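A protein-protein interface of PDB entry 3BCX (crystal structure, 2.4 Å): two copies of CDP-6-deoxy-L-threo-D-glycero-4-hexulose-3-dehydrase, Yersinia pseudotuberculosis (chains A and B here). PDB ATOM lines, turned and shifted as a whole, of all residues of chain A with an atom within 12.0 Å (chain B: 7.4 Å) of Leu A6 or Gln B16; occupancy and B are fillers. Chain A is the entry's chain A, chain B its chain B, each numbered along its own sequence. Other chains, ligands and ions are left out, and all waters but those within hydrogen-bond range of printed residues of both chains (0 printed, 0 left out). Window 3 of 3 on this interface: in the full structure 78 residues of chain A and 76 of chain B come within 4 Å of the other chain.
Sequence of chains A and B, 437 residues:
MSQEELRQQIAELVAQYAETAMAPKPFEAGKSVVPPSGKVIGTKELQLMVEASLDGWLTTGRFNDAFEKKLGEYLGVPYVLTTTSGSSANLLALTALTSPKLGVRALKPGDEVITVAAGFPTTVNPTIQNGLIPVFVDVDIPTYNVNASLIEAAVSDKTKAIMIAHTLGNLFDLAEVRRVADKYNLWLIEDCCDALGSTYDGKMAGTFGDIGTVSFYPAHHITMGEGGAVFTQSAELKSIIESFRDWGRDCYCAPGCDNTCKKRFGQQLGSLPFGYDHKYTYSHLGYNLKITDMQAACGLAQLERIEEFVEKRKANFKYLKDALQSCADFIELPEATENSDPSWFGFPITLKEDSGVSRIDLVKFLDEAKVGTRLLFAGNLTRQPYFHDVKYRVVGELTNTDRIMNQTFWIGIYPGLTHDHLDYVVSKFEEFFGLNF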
ATOM      1  N   SER A   2     -17.564  12.779  30.078  1.00  0.00           N
ATOM      2  CA  SER A   2     -17.038  13.839  30.988  1.00  0.00           C
ATOM      3  C   SER A   2     -18.006  15.012  31.109  1.00  0.00           C
ATOM      4  O   SER A   2     -18.693  15.367  30.147  1.00  0.00           O
ATOM      5  CB  SER A   2     -15.669  14.321  30.493  1.00  0.00           C
ATOM      6  OG  SER A   2     -15.598  14.298  29.081  1.00  0.00           O
ATOM      7  N   GLN A   3     -18.055  15.611  32.296  1.00  0.00           N
ATOM      8  CA  GLN A   3     -18.954  16.729  32.567  1.00  0.00           C
ATOM      9  C   GLN A   3     -18.551  18.030  31.883  1.00  0.00           C
ATOM     10  O   GLN A   3     -19.329  18.590  31.114  1.00  0.00           O
ATOM     11  CB  GLN A   3     -19.064  16.947  34.076  1.00  0.00           C
ATOM     12  CG  GLN A   3     -19.603  15.736  34.812  1.00  0.00           C
ATOM     13  CD  GLN A   3     -21.034  15.418  34.436  1.00  0.00           C
ATOM     14  OE1 GLN A   3     -21.964  16.088  34.876  1.00  0.00           O
ATOM     15  NE2 GLN A   3     -21.216  14.397  33.608  1.00  0.00           N
ATOM     16  N   GLU A   4     -17.345  18.513  32.164  1.00  0.00           N
ATOM     17  CA  GLU A   4     -16.877  19.750  31.553  1.00  0.00           C
ATOM     18  C   GLU A   4     -16.926  19.640  30.033  1.00  0.00           C
ATOM     19  O   GLU A   4     -16.979  20.644  29.322  1.00  0.00           O
ATOM     20  CB  GLU A   4     -15.448  20.060  32.004  1.00  0.00           C
ATOM     21  CG  GLU A   4     -14.796  21.222  31.265  1.00  0.00           C
ATOM     22  CD  GLU A   4     -15.558  22.530  31.415  1.00  0.00           C
ATOM     23  OE1 GLU A   4     -16.754  22.576  31.055  1.00  0.00           O
ATOM     24  OE2 GLU A   4     -14.958  23.515  31.890  1.00  0.00           O
ATOM     25  N   GLU A   5     -16.911  18.408  29.544  1.00  0.00           N
ATOM     26  CA  GLU A   5     -16.956  18.146  28.115  1.00  0.00           C
ATOM     27  C   GLU A   5     -18.388  18.250  27.598  1.00  0.00           C
ATOM     28  O   GLU A   5     -18.640  18.881  26.574  1.00  0.00           O
ATOM     29  CB  GLU A   5     -16.394  16.755  27.836  1.00  0.00           C
ATOM     30  CG  GLU A   5     -16.448  16.320  26.386  1.00  0.00           C
ATOM     31  CD  GLU A   5     -15.947  14.901  26.205  1.00  0.00           C
ATOM     32  OE1 GLU A   5     -14.763  14.645  26.520  1.00  0.00           O
ATOM     33  OE2 GLU A   5     -16.738  14.041  25.758  1.00  0.00           O
ATOM     34  N   LEU A   6     -19.321  17.625  28.311  1.00  0.00           N
ATOM     35  CA  LEU A   6     -20.724  17.665  27.923  1.00  0.00           C
ATOM     36  C   LEU A   6     -21.230  19.107  27.855  1.00  0.00           C
ATOM     37  O   LEU A   6     -22.057  19.440  27.009  1.00  0.00           O
ATOM     38  CB  LEU A   6     -21.574  16.857  28.911  1.00  0.00           C
ATOM     39  CG  LEU A   6     -21.569  15.335  28.751  1.00  0.00           C
ATOM     40  CD1 LEU A   6     -22.323  14.686  29.895  1.00  0.00           C
ATOM     41  CD2 LEU A   6     -22.209  14.966  27.425  1.00  0.00           C
ATOM     42  N   ARG A   7     -20.729  19.959  28.745  1.00  0.00           N
ATOM     43  CA  ARG A   7     -21.135  21.359  28.767  1.00  0.00           C
ATOM     44  C   ARG A   7     -20.708  22.083  27.497  1.00  0.00           C
ATOM     45  O   ARG A   7     -21.552  22.584  26.755  1.00  0.00           O
ATOM     46  CB  ARG A   7     -20.545  22.082  29.986  1.00  0.00           C
ATOM     47  CG  ARG A   7     -21.352  21.944  31.274  1.00  0.00           C
ATOM     48  CD  ARG A   7     -20.671  22.684  32.424  1.00  0.00           C
ATOM     49  NE  ARG A   7     -21.433  22.612  33.669  1.00  0.00           N
ATOM     50  CZ  ARG A   7     -22.447  23.413  33.989  1.00  0.00           C
ATOM     51  NH1 ARG A   7     -22.837  24.371  33.159  1.00  0.00           N
ATOM     52  NH2 ARG A   7     -23.080  23.252  35.141  1.00  0.00           N
ATOM     53  N   GLN A   8     -19.400  22.138  27.248  1.00  0.00           N
ATOM     54  CA  GLN A   8     -18.865  22.815  26.065  1.00  0.00           C
ATOM     55  C   GLN A   8     -19.536  22.374  24.771  1.00  0.00           C
ATOM     56  O   GLN A   8     -19.668  23.156  23.828  1.00  0.00           O
ATOM     57  CB  GLN A   8     -17.359  22.580  25.945  1.00  0.00           C
ATOM     58  CG  GLN A   8     -16.525  23.325  26.966  1.00  0.00           C
ATOM     59  CD  GLN A   8     -15.050  23.323  26.616  1.00  0.00           C
ATOM     60  OE1 GLN A   8     -14.229  23.898  27.329  1.00  0.00           O
ATOM     61  NE2 GLN A   8     -14.706  22.675  25.508  1.00  0.00           N
ATOM     62  N   GLN A   9     -19.954  21.115  24.737  1.00  0.00           N
ATOM     63  CA  GLN A   9     -20.607  20.543  23.571  1.00  0.00           C
ATOM     64  C   GLN A   9     -22.099  20.884  23.515  1.00  0.00           C
ATOM     65  O   GLN A   9     -22.724  20.814  22.456  1.00  0.00           O
ATOM     66  CB  GLN A   9     -20.357  19.030  23.567  1.00  0.00           C
ATOM     67  CG  GLN A   9     -21.493  18.160  23.089  1.00  0.00           C
ATOM     68  CD  GLN A   9     -21.071  16.709  22.973  1.00  0.00           C
ATOM     69  OE1 GLN A   9     -20.166  16.256  23.682  1.00  0.00           O
ATOM     70  NE2 GLN A   9     -21.727  15.969  22.087  1.00  0.00           N
ATOM     71  N   ILE A  10     -22.666  21.252  24.662  1.00  0.00           N
ATOM     72  CA  ILE A  10     -24.071  21.650  24.720  1.00  0.00           C
ATOM     73  C   ILE A  10     -24.077  23.114  24.305  1.00  0.00           C
ATOM     74  O   ILE A  10     -25.000  23.587  23.651  1.00  0.00           O
ATOM     75  CB  ILE A  10     -24.655  21.512  26.145  1.00  0.00           C
ATOM     76  CG1 ILE A  10     -24.856  20.029  26.480  1.00  0.00           C
ATOM     77  CG2 ILE A  10     -25.982  22.256  26.249  1.00  0.00           C
ATOM     78  CD1 ILE A  10     -25.398  19.774  27.874  1.00  0.00           C
ATOM     79  N   ALA A  11     -23.017  23.818  24.684  1.00  0.00           N
ATOM     80  CA  ALA A  11     -22.865  25.223  24.350  1.00  0.00           C
ATOM     81  C   ALA A  11     -22.846  25.379  22.832  1.00  0.00           C
ATOM     82  O   ALA A  11     -23.358  26.357  22.288  1.00  0.00           O
ATOM     83  CB  ALA A  11     -21.574  25.765  24.954  1.00  0.00           C
ATOM     84  N   GLU A  12     -22.257  24.399  22.157  1.00  0.00           N
ATOM     85  CA  GLU A  12     -22.155  24.409  20.701  1.00  0.00           C
ATOM     86  C   GLU A  12     -23.521  24.293  20.046  1.00  0.00           C
ATOM     87  O   GLU A  12     -23.887  25.113  19.211  1.00  0.00           O
ATOM     88  CB  GLU A  12     -21.269  23.254  20.228  1.00  0.00           C
ATOM     89  CG  GLU A  12     -19.896  23.219  20.872  1.00  0.00           C
ATOM     90  CD  GLU A  12     -19.083  24.472  20.603  1.00  0.00           C
ATOM     91  OE1 GLU A  12     -17.959  24.576  21.142  1.00  0.00           O
ATOM     92  OE2 GLU A  12     -19.561  25.351  19.854  1.00  0.00           O
ATOM     93  N   LEU A  13     -24.268  23.262  20.421  1.00  0.00           N
ATOM     94  CA  LEU A  13     -25.594  23.052  19.864  1.00  0.00           C
ATOM     95  C   LEU A  13     -26.522  24.226  20.173  1.00  0.00           C
ATOM     96  O   LEU A  13     -27.512  24.448  19.471  1.00  0.00           O
ATOM     97  CB  LEU A  13     -26.193  21.753  20.405  1.00  0.00           C
ATOM     98  CG  LEU A  13     -25.422  20.469  20.079  1.00  0.00           C
ATOM     99  CD1 LEU A  13     -26.223  19.266  20.556  1.00  0.00           C
ATOM    100  CD2 LEU A  13     -25.175  20.378  18.577  1.00  0.00           C
ATOM    101  N   VAL A  14     -26.200  24.970  21.227  1.00  0.00           N
ATOM    102  CA  VAL A  14     -26.996  26.125  21.615  1.00  0.00           C
ATOM    103  C   VAL A  14     -26.551  27.325  20.793  1.00  0.00           C
ATOM    104  O   VAL A  14     -27.377  28.095  20.304  1.00  0.00           O
ATOM    105  CB  VAL A  14     -26.832  26.447  23.121  1.00  0.00           C
ATOM    106  CG1 VAL A  14     -27.449  27.802  23.443  1.00  0.00           C
ATOM    107  CG2 VAL A  14     -27.498  25.368  23.953  1.00  0.00           C
ATOM    108  N   ALA A  15     -25.241  27.475  20.636  1.00  0.00           N
ATOM    109  CA  ALA A  15     -24.694  28.587  19.871  1.00  0.00           C
ATOM    110  C   ALA A  15     -25.114  28.502  18.409  1.00  0.00           C
ATOM    111  O   ALA A  15     -25.071  29.498  17.693  1.00  0.00           O
ATOM    112  CB  ALA A  15     -23.175  28.600  19.977  1.00  0.00           C
ATOM    113  N   GLN A  16     -25.526  27.314  17.974  1.00  0.00           N
ATOM    114  CA  GLN A  16     -25.945  27.102  16.593  1.00  0.00           C
ATOM    115  C   GLN A  16     -27.455  27.194  16.458  1.00  0.00           C
ATOM    116  O   GLN A  16     -27.979  27.403  15.365  1.00  0.00           O
ATOM    117  CB  GLN A  16     -25.452  25.739  16.098  1.00  0.00           C
ATOM    118  CG  GLN A  16     -23.932  25.592  16.145  1.00  0.00           C
ATOM    119  CD  GLN A  16     -23.461  24.161  15.932  1.00  0.00           C
ATOM    120  OE1 GLN A  16     -22.276  23.857  16.094  1.00  0.00           O
ATOM    121  NE2 GLN A  16     -24.387  23.274  15.565  1.00  0.00           N
ATOM    122  N   LEU A  46     -28.713  32.832  25.770  1.00  0.00           N
ATOM    123  CA  LEU A  46     -29.165  31.448  25.832  1.00  0.00           C
ATOM    124  C   LEU A  46     -28.097  30.497  26.360  1.00  0.00           C
ATOM    125  O   LEU A  46     -28.422  29.495  26.998  1.00  0.00           O
ATOM    126  CB  LEU A  46     -29.645  30.975  24.457  1.00  0.00           C
ATOM    127  CG  LEU A  46     -31.050  31.413  24.026  1.00  0.00           C
ATOM    128  CD1 LEU A  46     -31.104  32.933  23.883  1.00  0.00           C
ATOM    129  CD2 LEU A  46     -31.410  30.735  22.708  1.00  0.00           C
ATOM    130  N   GLN A  47     -26.829  30.807  26.103  1.00  0.00           N
ATOM    131  CA  GLN A  47     -25.748  29.953  26.574  1.00  0.00           C
ATOM    132  C   GLN A  47     -25.603  29.996  28.094  1.00  0.00           C
ATOM    133  O   GLN A  47     -25.564  28.946  28.740  1.00  0.00           O
ATOM    134  CB  GLN A  47     -24.424  30.339  25.908  1.00  0.00           C
ATOM    135  CG  GLN A  47     -24.333  29.933  24.438  1.00  0.00           C
ATOM    136  CD  GLN A  47     -22.911  29.975  23.900  1.00  0.00           C
ATOM    137  OE1 GLN A  47     -22.228  31.000  23.980  1.00  0.00           O
ATOM    138  NE2 GLN A  47     -22.460  28.854  23.342  1.00  0.00           N
ATOM    139  N   VAL A  50     -28.427  28.316  29.969  1.00  0.00           N
ATOM    140  CA  VAL A  50     -28.323  26.858  29.945  1.00  0.00           C
ATOM    141  C   VAL A  50     -27.312  26.448  31.013  1.00  0.00           C
ATOM    142  O   VAL A  50     -27.521  25.477  31.744  1.00  0.00           O
ATOM    143  CB  VAL A  50     -27.876  26.340  28.550  1.00  0.00           C
ATOM    144  CG1 VAL A  50     -27.495  24.857  28.625  1.00  0.00           C
ATOM    145  CG2 VAL A  50     -29.019  26.519  27.554  1.00  0.00           C
ATOM    146  N   GLU A  51     -26.224  27.205  31.108  1.00  0.00           N
ATOM    147  CA  GLU A  51     -25.207  26.924  32.110  1.00  0.00           C
ATOM    148  C   GLU A  51     -25.822  26.953  33.497  1.00  0.00           C
ATOM    149  O   GLU A  51     -25.675  25.999  34.268  1.00  0.00           O
ATOM    150  CB  GLU A  51     -24.082  27.941  32.023  1.00  0.00           C
ATOM    151  CG  GLU A  51     -23.169  27.666  30.873  1.00  0.00           C
ATOM    152  CD  GLU A  51     -21.718  27.787  31.268  1.00  0.00           C
ATOM    153  OE1 GLU A  51     -21.175  28.905  31.161  1.00  0.00           O
ATOM    154  OE2 GLU A  51     -21.133  26.769  31.702  1.00  0.00           O
ATOM    155  N   ALA A  52     -26.514  28.049  33.804  1.00  0.00           N
ATOM    156  CA  ALA A  52     -27.173  28.205  35.095  1.00  0.00           C
ATOM    157  C   ALA A  52     -28.140  27.047  35.337  1.00  0.00           C
ATOM    158  O   ALA A  52     -28.253  26.550  36.452  1.00  0.00           O
ATOM    159  CB  ALA A  52     -27.918  29.538  35.150  1.00  0.00           C
ATOM    160  N   SER A  53     -28.830  26.614  34.287  1.00  0.00           N
ATOM    161  CA  SER A  53     -29.784  25.513  34.409  1.00  0.00           C
ATOM    162  C   SER A  53     -29.056  24.230  34.788  1.00  0.00           C
ATOM    163  O   SER A  53     -29.515  23.464  35.641  1.00  0.00           O
ATOM    164  CB  SER A  53     -30.521  25.293  33.085  1.00  0.00           C
ATOM    165  OG  SER A  53     -31.127  26.486  32.629  1.00  0.00           O
ATOM    166  N   LEU A  54     -27.919  24.000  34.137  1.00  0.00           N
ATOM    167  CA  LEU A  54     -27.128  22.810  34.395  1.00  0.00           C
ATOM    168  C   LEU A  54     -26.571  22.823  35.813  1.00  0.00           C
ATOM    169  O   LEU A  54     -26.539  21.785  36.471  1.00  0.00           O
ATOM    170  CB  LEU A  54     -25.999  22.693  33.365  1.00  0.00           C
ATOM    171  CG  LEU A  54     -26.474  22.419  31.931  1.00  0.00           C
ATOM    172  CD1 LEU A  54     -25.287  22.413  30.981  1.00  0.00           C
ATOM    173  CD2 LEU A  54     -27.211  21.085  31.879  1.00  0.00           C
ATOM    174  N   ASP A  55     -26.144  23.997  36.280  1.00  0.00           N
ATOM    175  CA  ASP A  55     -25.613  24.136  37.636  1.00  0.00           C
ATOM    176  C   ASP A  55     -26.541  23.467  38.648  1.00  0.00           C
ATOM    177  O   ASP A  55     -26.084  22.836  39.602  1.00  0.00           O
ATOM    178  CB  ASP A  55     -25.459  25.612  38.020  1.00  0.00           C
ATOM    179  CG  ASP A  55     -24.288  26.283  37.330  1.00  0.00           C
ATOM    180  OD1 ASP A  55     -23.490  25.570  36.688  1.00  0.00           O
ATOM    181  OD2 ASP A  55     -24.161  27.523  37.441  1.00  0.00           O
ATOM    182  N   ARG A  62     -23.425  31.975  41.585  1.00  0.00           N
ATOM    183  CA  ARG A  62     -22.376  32.186  40.603  1.00  0.00           C
ATOM    184  C   ARG A  62     -22.682  33.313  39.595  1.00  0.00           C
ATOM    185  O   ARG A  62     -21.945  34.299  39.503  1.00  0.00           O
ATOM    186  CB  ARG A  62     -22.160  30.845  39.906  1.00  0.00           C
ATOM    187  CG  ARG A  62     -21.195  30.814  38.779  1.00  0.00           C
ATOM    188  CD  ARG A  62     -21.359  29.489  38.070  1.00  0.00           C
ATOM    189  NE  ARG A  62     -20.656  29.486  36.797  1.00  0.00           N
ATOM    190  CZ  ARG A  62     -20.892  28.618  35.823  1.00  0.00           C
ATOM    191  NH1 ARG A  62     -21.818  27.679  35.970  1.00  0.00           N
ATOM    192  NH2 ARG A  62     -20.196  28.693  34.698  1.00  0.00           N
ATOM    193  N   ILE B  10     -29.867  18.424  22.185  1.00  0.00           N
ATOM    194  CA  ILE B  10     -29.427  19.091  23.401  1.00  0.00           C
ATOM    195  C   ILE B  10     -30.081  18.373  24.576  1.00  0.00           C
ATOM    196  O   ILE B  10     -29.455  18.152  25.609  1.00  0.00           O
ATOM    197  CB  ILE B  10     -29.841  20.582  23.400  1.00  0.00           C
ATOM    198  CG1 ILE B  10     -29.047  21.333  22.328  1.00  0.00           C
ATOM    199  CG2 ILE B  10     -29.602  21.201  24.769  1.00  0.00           C
ATOM    200  CD1 ILE B  10     -29.392  22.803  22.211  1.00  0.00           C
ATOM    201  N   ALA B  11     -31.342  17.993  24.400  1.00  0.00           N
ATOM    202  CA  ALA B  11     -32.077  17.286  25.437  1.00  0.00           C
ATOM    203  C   ALA B  11     -31.300  16.046  25.878  1.00  0.00           C
ATOM    204  O   ALA B  11     -31.232  15.732  27.067  1.00  0.00           O
ATOM    205  CB  ALA B  11     -33.457  16.884  24.920  1.00  0.00           C
ATOM    206  N   GLU B  12     -30.712  15.348  24.911  1.00  0.00           N
ATOM    207  CA  GLU B  12     -29.951  14.137  25.188  1.00  0.00           C
ATOM    208  C   GLU B  12     -28.665  14.450  25.933  1.00  0.00           C
ATOM    209  O   GLU B  12     -28.337  13.790  26.913  1.00  0.00           O
ATOM    210  CB  GLU B  12     -29.616  13.411  23.880  1.00  0.00           C
ATOM    211  CG  GLU B  12     -30.822  13.111  23.007  1.00  0.00           C
ATOM    212  CD  GLU B  12     -31.848  12.229  23.693  1.00  0.00           C
ATOM    213  OE1 GLU B  12     -32.925  11.995  23.098  1.00  0.00           O
ATOM    214  OE2 GLU B  12     -31.577  11.768  24.823  1.00  0.00           O
ATOM    215  N   LEU B  13     -27.934  15.450  25.458  1.00  0.00           N
ATOM    216  CA  LEU B  13     -26.682  15.826  26.093  1.00  0.00           C
ATOM    217  C   LEU B  13     -26.854  16.274  27.539  1.00  0.00           C
ATOM    218  O   LEU B  13     -25.938  16.107  28.353  1.00  0.00           O
ATOM    219  CB  LEU B  13     -25.988  16.936  25.306  1.00  0.00           C
ATOM    220  CG  LEU B  13     -25.390  16.557  23.951  1.00  0.00           C
ATOM    221  CD1 LEU B  13     -24.674  17.769  23.387  1.00  0.00           C
ATOM    222  CD2 LEU B  13     -24.417  15.394  24.099  1.00  0.00           C
ATOM    223  N   VAL B  14     -28.010  16.851  27.870  1.00  0.00           N
ATOM    224  CA  VAL B  14     -28.241  17.285  29.247  1.00  0.00           C
ATOM    225  C   VAL B  14     -28.793  16.083  30.022  1.00  0.00           C
ATOM    226  O   VAL B  14     -28.593  15.984  31.232  1.00  0.00           O
ATOM    227  CB  VAL B  14     -29.256  18.475  29.334  1.00  0.00           C
ATOM    228  CG1 VAL B  14     -29.028  19.418  28.159  1.00  0.00           C
ATOM    229  CG2 VAL B  14     -30.684  17.968  29.387  1.00  0.00           C
ATOM    230  N   ALA B  15     -29.479  15.176  29.323  1.00  0.00           N
ATOM    231  CA  ALA B  15     -30.043  14.010  29.978  1.00  0.00           C
ATOM    232  C   ALA B  15     -28.948  13.116  30.554  1.00  0.00           C
ATOM    233  O   ALA B  15     -29.168  12.404  31.543  1.00  0.00           O
ATOM    234  CB  ALA B  15     -30.923  13.221  29.011  1.00  0.00           C
ATOM    235  N   GLN B  16     -27.775  13.125  29.928  1.00  0.00           N
ATOM    236  CA  GLN B  16     -26.677  12.299  30.408  1.00  0.00           C
ATOM    237  C   GLN B  16     -25.792  13.110  31.339  1.00  0.00           C
ATOM    238  O   GLN B  16     -25.010  12.551  32.105  1.00  0.00           O
ATOM    239  CB  GLN B  16     -25.856  11.751  29.234  1.00  0.00           C
ATOM    240  CG  GLN B  16     -24.825  12.710  28.672  1.00  0.00           C
ATOM    241  CD  GLN B  16     -23.877  12.024  27.707  1.00  0.00           C
ATOM    242  OE1 GLN B  16     -24.279  11.582  26.630  1.00  0.00           O
ATOM    243  NE2 GLN B  16     -22.611  11.917  28.098  1.00  0.00           N
ATOM    244  N   TYR B  17     -25.908  14.431  31.264  1.00  0.00           N
ATOM    245  CA  TYR B  17     -25.131  15.301  32.136  1.00  0.00           C
ATOM    246  C   TYR B  17     -25.767  15.205  33.518  1.00  0.00           C
ATOM    247  O   TYR B  17     -25.080  15.136  34.534  1.00  0.00           O
ATOM    248  CB  TYR B  17     -25.192  16.754  31.656  1.00  0.00           C
ATOM    249  CG  TYR B  17     -24.570  17.732  32.629  1.00  0.00           C
ATOM    250  CD1 TYR B  17     -23.244  18.134  32.494  1.00  0.00           C
ATOM    251  CD2 TYR B  17     -25.297  18.221  33.718  1.00  0.00           C
ATOM    252  CE1 TYR B  17     -22.654  18.995  33.417  1.00  0.00           C
ATOM    253  CE2 TYR B  17     -24.716  19.079  34.650  1.00  0.00           C
ATOM    254  CZ  TYR B  17     -23.396  19.463  34.494  1.00  0.00           C
ATOM    255  OH  TYR B  17     -22.815  20.310  35.414  1.00  0.00           O
ATOM    256  N   ALA B  18     -27.095  15.201  33.532  1.00  0.00           N
ATOM    257  CA  ALA B  18     -27.867  15.124  34.762  1.00  0.00           C
ATOM    258  C   ALA B  18     -27.697  13.778  35.466  1.00  0.00           C
ATOM    259  O   ALA B  18     -27.612  13.718  36.695  1.00  0.00           O
ATOM    260  CB  ALA B  18     -29.343  15.376  34.462  1.00  0.00           C
ATOM    261  N   GLU B  19     -27.647  12.697  34.692  1.00  0.00           N
ATOM    262  CA  GLU B  19     -27.490  11.367  35.271  1.00  0.00           C
ATOM    263  C   GLU B  19     -26.190  11.242  36.056  1.00  0.00           C
ATOM    264  O   GLU B  19     -26.071  10.405  36.948  1.00  0.00           O
ATOM    265  CB  GLU B  19     -27.557  10.304  34.177  1.00  0.00           C
ATOM    266  CG  GLU B  19     -28.953  10.123  33.618  1.00  0.00           C
ATOM    267  CD  GLU B  19     -28.985   9.220  32.406  1.00  0.00           C
ATOM    268  OE1 GLU B  19     -28.284   9.533  31.418  1.00  0.00           O
ATOM    269  OE2 GLU B  19     -29.711   8.202  32.439  1.00  0.00           O
ATOM    270  N   THR B  20     -25.220  12.086  35.728  1.00  0.00           N
ATOM    271  CA  THR B  20     -23.942  12.076  36.420  1.00  0.00           C
ATOM    272  C   THR B  20     -23.953  13.092  37.562  1.00  0.00           C
ATOM    273  O   THR B  20     -23.617  12.765  38.699  1.00  0.00           O
ATOM    274  CB  THR B  20     -22.787  12.417  35.458  1.00  0.00           C
ATOM    275  OG1 THR B  20     -22.676  11.391  34.464  1.00  0.00           O
ATOM    276  CG2 THR B  20     -21.475  12.532  36.215  1.00  0.00           C
ATOM    277  N   ALA B  21     -24.354  14.321  37.255  1.00  0.00           N
ATOM    278  CA  ALA B  21     -24.399  15.384  38.248  1.00  0.00           C
ATOM    279  C   ALA B  21     -25.452  15.157  39.334  1.00  0.00           C
ATOM    280  O   ALA B  21     -25.128  15.157  40.518  1.00  0.00           O
ATOM    281  CB  ALA B  21     -24.638  16.721  37.557  1.00  0.00           C
ATOM    282  N   THR B  43     -33.140  15.005  35.694  1.00  0.00           N
ATOM    283  CA  THR B  43     -33.071  15.254  34.259  1.00  0.00           C
ATOM    284  C   THR B  43     -34.213  16.116  33.732  1.00  0.00           C
ATOM    285  O   THR B  43     -33.984  17.066  32.990  1.00  0.00           O
ATOM    286  CB  THR B  43     -33.052  13.927  33.473  1.00  0.00           C
ATOM    287  OG1 THR B  43     -31.893  13.173  33.851  1.00  0.00           O
ATOM    288  CG2 THR B  43     -33.021  14.194  31.963  1.00  0.00           C
ATOM    289  N   GLN B  47     -33.899  19.631  31.823  1.00  0.00           N
ATOM    290  CA  GLN B  47     -34.323  19.609  30.433  1.00  0.00           C
ATOM    291  C   GLN B  47     -35.310  20.727  30.097  1.00  0.00           C
ATOM    292  O   GLN B  47     -35.116  21.447  29.114  1.00  0.00           O
ATOM    293  CB  GLN B  47     -34.927  18.247  30.071  1.00  0.00           C
ATOM    294  CG  GLN B  47     -33.899  17.119  29.981  1.00  0.00           C
ATOM    295  CD  GLN B  47     -34.466  15.848  29.371  1.00  0.00           C
ATOM    296  OE1 GLN B  47     -35.508  15.349  29.796  1.00  0.00           O
ATOM    297  NE2 GLN B  47     -33.771  15.312  28.369  1.00  0.00           N
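The side-chain amide oxygen (OE1) of Gln A3 lies close to the backbone carbonyl oxygen (O) of Tyr B17 (3.3 Å). The side-chain amide nitrogen (NE2) of Gln A3 sits close to the side-chain hydroxyl (OG1) of Thr B20 (3.4 Å). The side-chain hydroxyl of Tyr B17 lies within hydrogen-bond range of the guanidinium group of Arg A7 (3.0 Å).
The guanidinium group of Arg A7 lies within salt-bridge range of the side-chain carboxylate of Glu A51, 3.3 Å away. The guanidinium group of Arg A7 is in salt-bridge range of the side-chain carboxylate of Asp A55 (2.8 Å).
Among the printed residues, merely in contact across the chains: Leu A6 with Gln B16, Gln A9 with Leu B13, Leu A13 with Ile B10, Ile A10 with Leu B13, Leu A13 with Leu B13, Val A14 with Ile B10, Leu A6 with Tyr B17, Ile A10 with Val B14, Leu A54 with Tyr B17 and Gln A3 with Ala B21.
Of the printed residues of chain B, Gln A9 touches Leu B13. Printed residues of chain B within 4 Å of Ile A10: Leu B13 (3.5 Å) and Val B14 (3.7 Å). Printed residues of chain B within 4 Å of Leu A13: Ile B10 (3.5 Å) and Leu B13 (3.6 Å). Printed residues of chain A within 4 Å of Ile B10: Leu A13 (3.5 Å) and Val A14 (3.6 Å). Of the printed residues of chain A, Leu B13 touches Gln A9 (3.2 Å), Ile A10 (3.5 Å) and Leu A13 (3.6 Å). Val B14 touches just one residue of chain A: Ile A10 (3.7 Å). Gln B16 touches one residue of chain A. Printed residues of chain A within 4 Å of Tyr B17: Gln A3 (3.3 Å), Leu A6 (3.6 Å), Arg A7 (3.0 Å) and Leu A54 (3.7 Å). No residue of chain A comes within 4 Å of Ala B18. No residue of chain A comes within 4 Å of Glu B19. Thr B20 touches just one residue of chain A: Gln A3. The nearest printed residue of chain B that does not touch Leu A6 is Leu B13 (4.01 Å). The nearest residue of chain A that does not touch Gln B16 is Gln A3 (4.5 Å). The nearest printed residue of chain B that does not touch Ile A10 is Ile B10 (4.1 Å).
Printed residues of chain A that touch a printed residue of chain B: Gln A3, Leu A6, Arg A7, Gln A9, Ile A10, Leu A13, Val A14 and Leu A54. Of the 14 printed residues of chain B, 7 touch a printed residue of chain A. Among the printed residues, 13 pairs touch across the chains. Among the printed residues, no Asp or Glu carboxylate lies within 4 Å of a Lys or Arg side-chain nitrogen of the other chain.
Ile A10 touches Leu B13, and with the chains exchanged Leu A13 touches Ile B10. Ile A10 touches Val B14, and with the chains exchanged Val A14 touches Ile B10. Leu A13 touches its own counterpart, Leu B13.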
